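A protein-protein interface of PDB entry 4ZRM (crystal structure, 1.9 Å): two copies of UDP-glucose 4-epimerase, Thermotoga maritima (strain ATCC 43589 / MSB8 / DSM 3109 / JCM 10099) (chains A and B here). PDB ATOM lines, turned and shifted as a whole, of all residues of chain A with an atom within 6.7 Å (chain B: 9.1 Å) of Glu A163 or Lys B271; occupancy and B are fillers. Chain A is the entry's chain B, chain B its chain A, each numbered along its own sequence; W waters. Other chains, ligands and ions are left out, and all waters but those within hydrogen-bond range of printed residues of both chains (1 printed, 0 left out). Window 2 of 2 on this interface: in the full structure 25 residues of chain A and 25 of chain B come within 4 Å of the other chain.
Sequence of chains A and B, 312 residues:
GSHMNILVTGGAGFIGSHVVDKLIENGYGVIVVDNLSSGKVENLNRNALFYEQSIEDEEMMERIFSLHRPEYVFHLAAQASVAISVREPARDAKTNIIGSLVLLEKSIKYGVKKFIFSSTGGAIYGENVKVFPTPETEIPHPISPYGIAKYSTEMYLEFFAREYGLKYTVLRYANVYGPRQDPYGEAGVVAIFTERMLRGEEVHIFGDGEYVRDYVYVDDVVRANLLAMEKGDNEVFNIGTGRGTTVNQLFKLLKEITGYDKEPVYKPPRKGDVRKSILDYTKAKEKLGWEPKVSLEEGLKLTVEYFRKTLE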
ATOM      1  N   GLU A 158     -21.473  33.744   4.725  1.00  0.00           N
ATOM      2  CA  GLU A 158     -22.617  32.961   4.286  1.00  0.00           C
ATOM      3  C   GLU A 158     -22.177  31.641   3.661  1.00  0.00           C
ATOM      4  O   GLU A 158     -22.823  30.613   3.869  1.00  0.00           O
ATOM      5  CB  GLU A 158     -23.507  33.758   3.321  1.00  0.00           C
ATOM      6  CG  GLU A 158     -24.699  32.973   2.784  1.00  0.00           C
ATOM      7  CD  GLU A 158     -25.665  32.480   3.870  1.00  0.00           C
ATOM      8  OE1 GLU A 158     -25.851  33.173   4.901  1.00  0.00           O
ATOM      9  OE2 GLU A 158     -26.250  31.386   3.678  1.00  0.00           O
ATOM     10  N   PHE A 159     -21.077  31.658   2.913  1.00  0.00           N
ATOM     11  CA  PHE A 159     -20.534  30.414   2.371  1.00  0.00           C
ATOM     12  C   PHE A 159     -20.150  29.435   3.484  1.00  0.00           C
ATOM     13  O   PHE A 159     -20.546  28.270   3.444  1.00  0.00           O
ATOM     14  CB  PHE A 159     -19.316  30.669   1.460  1.00  0.00           C
ATOM     15  CG  PHE A 159     -18.398  29.473   1.332  1.00  0.00           C
ATOM     16  CD1 PHE A 159     -18.751  28.404   0.518  1.00  0.00           C
ATOM     17  CD2 PHE A 159     -17.199  29.406   2.042  1.00  0.00           C
ATOM     18  CE1 PHE A 159     -17.928  27.285   0.407  1.00  0.00           C
ATOM     19  CE2 PHE A 159     -16.369  28.288   1.938  1.00  0.00           C
ATOM     20  CZ  PHE A 159     -16.735  27.226   1.117  1.00  0.00           C
ATOM     21  N   PHE A 160     -19.389  29.888   4.479  1.00  0.00           N
ATOM     22  CA  PHE A 160     -18.966  28.959   5.540  1.00  0.00           C
ATOM     23  C   PHE A 160     -20.156  28.394   6.310  1.00  0.00           C
ATOM     24  O   PHE A 160     -20.128  27.230   6.730  1.00  0.00           O
ATOM     25  CB  PHE A 160     -17.939  29.580   6.502  1.00  0.00           C
ATOM     26  CG  PHE A 160     -16.549  29.693   5.920  1.00  0.00           C
ATOM     27  CD1 PHE A 160     -15.623  28.666   6.085  1.00  0.00           C
ATOM     28  CD2 PHE A 160     -16.174  30.822   5.203  1.00  0.00           C
ATOM     29  CE1 PHE A 160     -14.344  28.768   5.546  1.00  0.00           C
ATOM     30  CE2 PHE A 160     -14.900  30.930   4.652  1.00  0.00           C
ATOM     31  CZ  PHE A 160     -13.981  29.907   4.830  1.00  0.00           C
ATOM     32  N   ALA A 161     -21.194  29.204   6.494  1.00  0.00           N
ATOM     33  CA  ALA A 161     -22.407  28.724   7.157  1.00  0.00           C
ATOM     34  C   ALA A 161     -23.078  27.620   6.341  1.00  0.00           C
ATOM     35  O   ALA A 161     -23.475  26.583   6.886  1.00  0.00           O
ATOM     36  CB  ALA A 161     -23.386  29.882   7.392  1.00  0.00           C
ATOM     37  N   ARG A 162     -23.224  27.848   5.037  1.00  0.00           N
ATOM     38  CA  ARG A 162     -23.873  26.875   4.162  1.00  0.00           C
ATOM     39  C   ARG A 162     -23.043  25.616   4.013  1.00  0.00           C
ATOM     40  O   ARG A 162     -23.579  24.501   3.958  1.00  0.00           O
ATOM     41  CB  ARG A 162     -24.108  27.472   2.772  1.00  0.00           C
ATOM     42  CG  ARG A 162     -25.150  28.573   2.721  1.00  0.00           C
ATOM     43  CD  ARG A 162     -25.027  29.299   1.391  1.00  0.00           C
ATOM     44  NE  ARG A 162     -24.763  28.345   0.319  1.00  0.00           N
ATOM     45  CZ  ARG A 162     -25.715  27.761  -0.400  1.00  0.00           C
ATOM     46  NH1 ARG A 162     -26.988  28.052  -0.163  1.00  0.00           N
ATOM     47  NH2 ARG A 162     -25.398  26.896  -1.356  1.00  0.00           N
ATOM     48  N   GLU A 163     -21.729  25.793   3.928  1.00  0.00           N
ATOM     49  CA  GLU A 163     -20.833  24.673   3.657  1.00  0.00           C
ATOM     50  C   GLU A 163     -20.590  23.787   4.883  1.00  0.00           C
ATOM     51  O   GLU A 163     -20.497  22.567   4.753  1.00  0.00           O
ATOM     52  CB  GLU A 163     -19.496  25.181   3.086  1.00  0.00           C
ATOM     53  CG  GLU A 163     -18.533  24.079   2.616  1.00  0.00           C
ATOM     54  CD  GLU A 163     -18.949  23.448   1.287  1.00  0.00           C
ATOM     55  OE1 GLU A 163     -18.435  22.356   0.947  1.00  0.00           O
ATOM     56  OE2 GLU A 163     -19.784  24.046   0.580  1.00  0.00           O
ATOM     57  N   TYR A 164     -20.504  24.393   6.068  1.00  0.00           N
ATOM     58  CA  TYR A 164     -20.097  23.666   7.261  1.00  0.00           C
ATOM     59  C   TYR A 164     -21.034  23.809   8.452  1.00  0.00           C
ATOM     60  O   TYR A 164     -20.822  23.181   9.480  1.00  0.00           O
ATOM     61  CB  TYR A 164     -18.704  24.110   7.716  1.00  0.00           C
ATOM     62  CG  TYR A 164     -17.635  23.967   6.665  1.00  0.00           C
ATOM     63  CD1 TYR A 164     -17.104  22.720   6.352  1.00  0.00           C
ATOM     64  CD2 TYR A 164     -17.160  25.073   5.984  1.00  0.00           C
ATOM     65  CE1 TYR A 164     -16.122  22.581   5.391  1.00  0.00           C
ATOM     66  CE2 TYR A 164     -16.170  24.947   5.015  1.00  0.00           C
ATOM     67  CZ  TYR A 164     -15.658  23.697   4.728  1.00  0.00           C
ATOM     68  OH  TYR A 164     -14.683  23.557   3.767  1.00  0.00           O
ATOM     69  N   GLY A 165     -22.041  24.655   8.340  1.00  0.00           N
ATOM     70  CA  GLY A 165     -22.964  24.823   9.446  1.00  0.00           C
ATOM     71  C   GLY A 165     -22.440  25.756  10.519  1.00  0.00           C
ATOM     72  O   GLY A 165     -22.957  25.768  11.630  1.00  0.00           O
ATOM     73  N   LEU A 166     -21.412  26.538  10.202  1.00  0.00           N
ATOM     74  CA  LEU A 166     -20.920  27.533  11.153  1.00  0.00           C
ATOM     75  C   LEU A 166     -22.025  28.561  11.349  1.00  0.00           C
ATOM     76  O   LEU A 166     -22.650  28.989  10.394  1.00  0.00           O
ATOM     77  CB  LEU A 166     -19.644  28.217  10.633  1.00  0.00           C
ATOM     78  CG  LEU A 166     -19.070  29.358  11.493  1.00  0.00           C
ATOM     79  CD1 LEU A 166     -18.654  28.853  12.861  1.00  0.00           C
ATOM     80  CD2 LEU A 166     -17.892  30.009  10.799  1.00  0.00           C
ATOM     81  N   VAL B  82     -13.757  25.639  -9.162  1.00  0.00           N
ATOM     82  CA  VAL B  82     -14.664  25.921  -8.057  1.00  0.00           C
ATOM     83  C   VAL B  82     -14.382  25.020  -6.855  1.00  0.00           C
ATOM     84  O   VAL B  82     -14.366  25.478  -5.712  1.00  0.00           O
ATOM     85  CB  VAL B  82     -16.140  25.807  -8.470  1.00  0.00           C
ATOM     86  CG1 VAL B  82     -17.035  26.142  -7.290  1.00  0.00           C
ATOM     87  CG2 VAL B  82     -16.437  26.759  -9.623  1.00  0.00           C
ATOM     88  N   ALA B  83     -14.140  23.741  -7.117  1.00  0.00           N
ATOM     89  CA  ALA B  83     -13.890  22.796  -6.030  1.00  0.00           C
ATOM     90  C   ALA B  83     -12.649  23.145  -5.212  1.00  0.00           C
ATOM     91  O   ALA B  83     -12.635  22.982  -3.981  1.00  0.00           O
ATOM     92  CB  ALA B  83     -13.777  21.381  -6.586  1.00  0.00           C
ATOM     93  N   SER B  85     -11.509  26.170  -4.832  1.00  0.00           N
ATOM     94  CA  SER B  85     -11.834  27.381  -4.067  1.00  0.00           C
ATOM     95  C   SER B  85     -12.584  27.038  -2.785  1.00  0.00           C
ATOM     96  O   SER B  85     -12.435  27.715  -1.776  1.00  0.00           O
ATOM     97  CB  SER B  85     -12.642  28.378  -4.905  1.00  0.00           C
ATOM     98  OG  SER B  85     -14.031  28.063  -4.932  1.00  0.00           O
ATOM     99  N   VAL B  86     -13.378  25.978  -2.833  1.00  0.00           N
ATOM    100  CA  VAL B  86     -14.127  25.533  -1.666  1.00  0.00           C
ATOM    101  C   VAL B  86     -13.198  24.942  -0.605  1.00  0.00           C
ATOM    102  O   VAL B  86     -13.335  25.237   0.590  1.00  0.00           O
ATOM    103  CB  VAL B  86     -15.208  24.515  -2.075  1.00  0.00           C
ATOM    104  CG1 VAL B  86     -15.818  23.845  -0.848  1.00  0.00           C
ATOM    105  CG2 VAL B  86     -16.286  25.210  -2.905  1.00  0.00           C
ATOM    106  N   ARG B  87     -12.247  24.123  -1.047  1.00  0.00           N
ATOM    107  CA  ARG B  87     -11.275  23.513  -0.141  1.00  0.00           C
ATOM    108  C   ARG B  87     -10.259  24.520   0.420  1.00  0.00           C
ATOM    109  O   ARG B  87      -9.812  24.386   1.572  1.00  0.00           O
ATOM    110  CB  ARG B  87     -10.549  22.364  -0.855  1.00  0.00           C
ATOM    111  CG  ARG B  87      -9.664  21.521   0.049  1.00  0.00           C
ATOM    112  CD  ARG B  87      -9.153  20.275  -0.669  1.00  0.00           C
ATOM    113  NE  ARG B  87     -10.224  19.367  -1.083  1.00  0.00           N
ATOM    114  CZ  ARG B  87     -10.812  18.470  -0.285  1.00  0.00           C
ATOM    115  NH1 ARG B  87     -10.456  18.370   0.993  1.00  0.00           N
ATOM    116  NH2 ARG B  87     -11.769  17.679  -0.765  1.00  0.00           N
ATOM    117  N   PRO B  89     -10.267  28.454   0.477  1.00  0.00           N
ATOM    118  CA  PRO B  89     -10.813  29.775   0.135  1.00  0.00           C
ATOM    119  C   PRO B  89      -9.781  30.885   0.287  1.00  0.00           C
ATOM    120  O   PRO B  89      -9.767  31.804  -0.536  1.00  0.00           O
ATOM    121  CB  PRO B  89     -11.951  29.987   1.149  1.00  0.00           C
ATOM    122  CG  PRO B  89     -12.110  28.695   1.888  1.00  0.00           C
ATOM    123  CD  PRO B  89     -10.923  27.834   1.644  1.00  0.00           C
ATOM    124  N   GLU B 127     -28.046  30.770  -6.793  1.00  0.00           N
ATOM    125  CA  GLU B 127     -28.832  29.547  -6.941  1.00  0.00           C
ATOM    126  C   GLU B 127     -30.342  29.766  -6.967  1.00  0.00           C
ATOM    127  O   GLU B 127     -31.101  28.795  -6.996  1.00  0.00           O
ATOM    128  CB  GLU B 127     -28.473  28.554  -5.832  1.00  0.00           C
ATOM    129  CG  GLU B 127     -28.863  29.028  -4.446  1.00  0.00           C
ATOM    130  CD  GLU B 127     -28.418  28.069  -3.346  1.00  0.00           C
ATOM    131  OE1 GLU B 127     -28.667  28.378  -2.159  1.00  0.00           O
ATOM    132  OE2 GLU B 127     -27.819  27.015  -3.661  1.00  0.00           O
ATOM    133  N   ILE B 143     -22.306  31.892  -4.341  1.00  0.00           N
ATOM    134  CA  ILE B 143     -22.337  30.935  -3.239  1.00  0.00           C
ATOM    135  C   ILE B 143     -21.025  30.175  -3.041  1.00  0.00           C
ATOM    136  O   ILE B 143     -20.876  29.442  -2.062  1.00  0.00           O
ATOM    137  CB  ILE B 143     -23.464  29.904  -3.434  1.00  0.00           C
ATOM    138  CG1 ILE B 143     -23.211  29.061  -4.690  1.00  0.00           C
ATOM    139  CG2 ILE B 143     -24.802  30.606  -3.515  1.00  0.00           C
ATOM    140  CD1 ILE B 143     -24.196  27.916  -4.888  1.00  0.00           C
ATOM    141  N   SER B 144     -20.087  30.316  -3.974  1.00  0.00           N
ATOM    142  CA  SER B 144     -18.782  29.660  -3.829  1.00  0.00           C
ATOM    143  C   SER B 144     -17.707  30.716  -3.637  1.00  0.00           C
ATOM    144  O   SER B 144     -17.892  31.864  -4.032  1.00  0.00           O
ATOM    145  CB  SER B 144     -18.450  28.810  -5.053  1.00  0.00           C
ATOM    146  OG  SER B 144     -18.244  29.621  -6.203  1.00  0.00           O
ATOM    147  N   PRO B 145     -16.578  30.336  -3.025  1.00  0.00           N
ATOM    148  CA  PRO B 145     -15.503  31.315  -2.833  1.00  0.00           C
ATOM    149  C   PRO B 145     -15.026  31.885  -4.163  1.00  0.00           C
ATOM    150  O   PRO B 145     -14.752  33.081  -4.259  1.00  0.00           O
ATOM    151  CB  PRO B 145     -14.412  30.483  -2.151  1.00  0.00           C
ATOM    152  CG  PRO B 145     -15.198  29.465  -1.357  1.00  0.00           C
ATOM    153  CD  PRO B 145     -16.296  29.069  -2.324  1.00  0.00           C
ATOM    154  N   PHE B 206     -23.248  13.228 -11.961  1.00  0.00           N
ATOM    155  CA  PHE B 206     -23.645  13.502 -10.583  1.00  0.00           C
ATOM    156  C   PHE B 206     -25.114  13.843 -10.491  1.00  0.00           C
ATOM    157  O   PHE B 206     -25.667  14.480 -11.395  1.00  0.00           O
ATOM    158  CB  PHE B 206     -22.785  14.618 -10.002  1.00  0.00           C
ATOM    159  CG  PHE B 206     -21.321  14.338 -10.121  1.00  0.00           C
ATOM    160  CD1 PHE B 206     -20.766  13.248  -9.466  1.00  0.00           C
ATOM    161  CD2 PHE B 206     -20.508  15.132 -10.915  1.00  0.00           C
ATOM    162  CE1 PHE B 206     -19.417  12.962  -9.590  1.00  0.00           C
ATOM    163  CE2 PHE B 206     -19.161  14.854 -11.040  1.00  0.00           C
ATOM    164  CZ  PHE B 206     -18.615  13.764 -10.381  1.00  0.00           C
ATOM    165  N   GLY B 207     -25.755  13.391  -9.415  1.00  0.00           N
ATOM    166  CA  GLY B 207     -27.183  13.594  -9.255  1.00  0.00           C
ATOM    167  C   GLY B 207     -27.977  12.973 -10.393  1.00  0.00           C
ATOM    168  O   GLY B 207     -27.672  11.856 -10.832  1.00  0.00           O
ATOM    169  N   TYR B 211     -28.779  19.051 -14.443  1.00  0.00           N
ATOM    170  CA  TYR B 211     -28.182  20.382 -14.291  1.00  0.00           C
ATOM    171  C   TYR B 211     -27.952  21.050 -15.641  1.00  0.00           C
ATOM    172  O   TYR B 211     -27.334  20.472 -16.536  1.00  0.00           O
ATOM    173  CB  TYR B 211     -26.864  20.279 -13.524  1.00  0.00           C
ATOM    174  CG  TYR B 211     -27.063  19.668 -12.160  1.00  0.00           C
ATOM    175  CD1 TYR B 211     -27.273  20.473 -11.042  1.00  0.00           C
ATOM    176  CD2 TYR B 211     -27.088  18.283 -11.994  1.00  0.00           C
ATOM    177  CE1 TYR B 211     -27.479  19.914  -9.786  1.00  0.00           C
ATOM    178  CE2 TYR B 211     -27.293  17.716 -10.748  1.00  0.00           C
ATOM    179  CZ  TYR B 211     -27.484  18.536  -9.648  1.00  0.00           C
ATOM    180  OH  TYR B 211     -27.686  17.971  -8.410  1.00  0.00           O
ATOM    181  N   ARG B 213     -26.507  24.065 -18.118  1.00  0.00           N
ATOM    182  CA  ARG B 213     -25.447  25.059 -18.293  1.00  0.00           C
ATOM    183  C   ARG B 213     -25.500  25.643 -19.697  1.00  0.00           C
ATOM    184  O   ARG B 213     -26.165  25.105 -20.574  1.00  0.00           O
ATOM    185  CB  ARG B 213     -24.061  24.435 -18.066  1.00  0.00           C
ATOM    186  CG  ARG B 213     -23.816  23.917 -16.638  1.00  0.00           C
ATOM    187  CD  ARG B 213     -23.795  25.052 -15.625  1.00  0.00           C
ATOM    188  NE  ARG B 213     -23.497  24.559 -14.279  1.00  0.00           N
ATOM    189  CZ  ARG B 213     -24.420  24.215 -13.388  1.00  0.00           C
ATOM    190  NH1 ARG B 213     -25.704  24.338 -13.686  1.00  0.00           N
ATOM    191  NH2 ARG B 213     -24.061  23.770 -12.192  1.00  0.00           N
ATOM    192  N   PRO B 268     -23.957  10.129  -6.419  1.00  0.00           N
ATOM    193  CA  PRO B 268     -24.620  11.128  -5.574  1.00  0.00           C
ATOM    194  C   PRO B 268     -24.260  12.552  -5.990  1.00  0.00           C
ATOM    195  O   PRO B 268     -23.162  12.793  -6.515  1.00  0.00           O
ATOM    196  CB  PRO B 268     -24.057  10.831  -4.177  1.00  0.00           C
ATOM    197  CG  PRO B 268     -23.735   9.372  -4.211  1.00  0.00           C
ATOM    198  CD  PRO B 268     -23.241   9.115  -5.618  1.00  0.00           C
ATOM    199  N   PRO B 269     -25.185  13.498  -5.775  1.00  0.00           N
ATOM    200  CA  PRO B 269     -24.938  14.868  -6.226  1.00  0.00           C
ATOM    201  C   PRO B 269     -23.831  15.521  -5.410  1.00  0.00           C
ATOM    202  O   PRO B 269     -23.595  15.159  -4.250  1.00  0.00           O
ATOM    203  CB  PRO B 269     -26.281  15.571  -5.977  1.00  0.00           C
ATOM    204  CG  PRO B 269     -26.937  14.764  -4.898  1.00  0.00           C
ATOM    205  CD  PRO B 269     -26.500  13.345  -5.127  1.00  0.00           C
ATOM    206  N   ARG B 270     -23.144  16.479  -6.012  1.00  0.00           N
ATOM    207  CA  ARG B 270     -22.088  17.170  -5.290  1.00  0.00           C
ATOM    208  C   ARG B 270     -22.627  18.453  -4.694  1.00  0.00           C
ATOM    209  O   ARG B 270     -23.576  19.035  -5.204  1.00  0.00           O
ATOM    210  CB  ARG B 270     -20.867  17.395  -6.187  1.00  0.00           C
ATOM    211  CG  ARG B 270     -19.956  16.158  -6.234  1.00  0.00           C
ATOM    212  CD  ARG B 270     -18.874  16.234  -7.302  1.00  0.00           C
ATOM    213  NE  ARG B 270     -17.967  15.089  -7.218  1.00  0.00           N
ATOM    214  CZ  ARG B 270     -16.876  14.943  -7.964  1.00  0.00           C
ATOM    215  NH1 ARG B 270     -16.558  15.874  -8.854  1.00  0.00           N
ATOM    216  NH2 ARG B 270     -16.107  13.867  -7.829  1.00  0.00           N
ATOM    217  N   LYS B 271     -22.037  18.867  -3.586  1.00  0.00           N
ATOM    218  CA  LYS B 271     -22.462  20.061  -2.884  1.00  0.00           C
ATOM    219  C   LYS B 271     -22.209  21.273  -3.778  1.00  0.00           C
ATOM    220  O   LYS B 271     -21.220  21.306  -4.499  1.00  0.00           O
ATOM    221  CB  LYS B 271     -21.617  20.179  -1.625  1.00  0.00           C
ATOM    222  CG  LYS B 271     -22.288  20.767  -0.434  1.00  0.00           C
ATOM    223  CD  LYS B 271     -21.572  20.236   0.783  1.00  0.00           C
ATOM    224  CE  LYS B 271     -21.839  21.063   2.011  1.00  0.00           C
ATOM    225  NZ  LYS B 271     -20.975  20.535   3.116  1.00  0.00           N
ATOM    226  N   GLY B 272     -23.108  22.251  -3.746  1.00  0.00           N
ATOM    227  CA  GLY B 272     -22.861  23.524  -4.400  1.00  0.00           C
ATOM    228  C   GLY B 272     -23.154  23.590  -5.885  1.00  0.00           C
ATOM    229  O   GLY B 272     -22.834  24.585  -6.534  1.00  0.00           O
ATOM    230  N   ASP B 273     -23.758  22.541  -6.429  1.00  0.00           N
ATOM    231  CA  ASP B 273     -24.054  22.472  -7.856  1.00  0.00           C
ATOM    232  C   ASP B 273     -25.330  23.276  -8.187  1.00  0.00           C
ATOM    233  O   ASP B 273     -26.439  22.821  -7.918  1.00  0.00           O
ATOM    234  CB  ASP B 273     -24.243  21.003  -8.249  1.00  0.00           C
ATOM    235  CG  ASP B 273     -23.751  20.690  -9.650  1.00  0.00           C
ATOM    236  OD1 ASP B 273     -23.678  21.621 -10.481  1.00  0.00           O
ATOM    237  OD2 ASP B 273     -23.449  19.502  -9.922  1.00  0.00           O
ATOM    238  N   VAL B 274     -25.173  24.463  -8.767  1.00  0.00           N
ATOM    239  CA  VAL B 274     -26.316  25.292  -9.177  1.00  0.00           C
ATOM    240  C   VAL B 274     -27.192  24.535 -10.180  1.00  0.00           C
ATOM    241  O   VAL B 274     -26.675  23.891 -11.090  1.00  0.00           O
ATOM    242  CB  VAL B 274     -25.831  26.637  -9.782  1.00  0.00           C
ATOM    243  CG1 VAL B 274     -26.982  27.416 -10.406  1.00  0.00           C
ATOM    244  CG2 VAL B 274     -25.140  27.481  -8.710  1.00  0.00           C
HETATM  245  O   HOH W   1     -13.351  25.645   3.150  1.00  0.00           O
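No position is printed for both chains. Of the 9 pairs that touch across the chains among the printed residues, none has its exchanged pair printed and touching as well.
The side-chain amino group of Lys B271 lies within salt-bridge range of the side-chain carboxylate of Glu A163 (3.8 Å). The side-chain carboxylate of Glu B127 is in salt-bridge range of the guanidinium group of Arg A162 (2.6 Å).
Of the printed residues of chain B, Phe A159 touches Val B86 (3.97 Å), Ile B143 (3.5 Å) and Pro B145 (3.6 Å). Of chain B, only Val B86 (3.5 Å) and Lys B271 (2.7 Å) come within 4 Å of Glu A163. Of chain B, only Val B86 (3.8 Å) comes within 4 Å of Tyr A164. Of the printed residues of chain A, Val B86 touches Phe A159 (3.97 Å), Glu A163 (3.5 Å) and Tyr A164 (3.8 Å). Of the printed residues of chain A, Glu B127 touches Arg A162. The nearest residue of chain B that does not touch Glu A163 is Gly B272 (5.7 Å).
Printed residues of chain B that touch a printed residue of chain A: Val B86, Pro B89, Glu B127, Ile B143, Pro B145 and Lys B271. Hydrophobic or aromatic side chains of chain B within 4 Å of the printed part of chain A: Val B86, Pro B89, Ile B143 and Pro B145.
Among the printed residues, merely in contact across the chains: Phe A159 with Val B86 (3.97 Å), Phe A159 with Ile B143 (3.5 Å), Phe A159 with Pro B145 (3.6 Å), Phe A160 with Pro B89 (3.7 Å), Arg A162 with Ile B143 (3.9 Å), Glu A163 with Val B86 (3.5 Å) and Tyr A164 with Val B86 (3.8 Å).
Water W1 lies within hydrogen-bond range of OH of Tyr A164 (2.6 Å) and O of Val B86 (2.6 Å).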
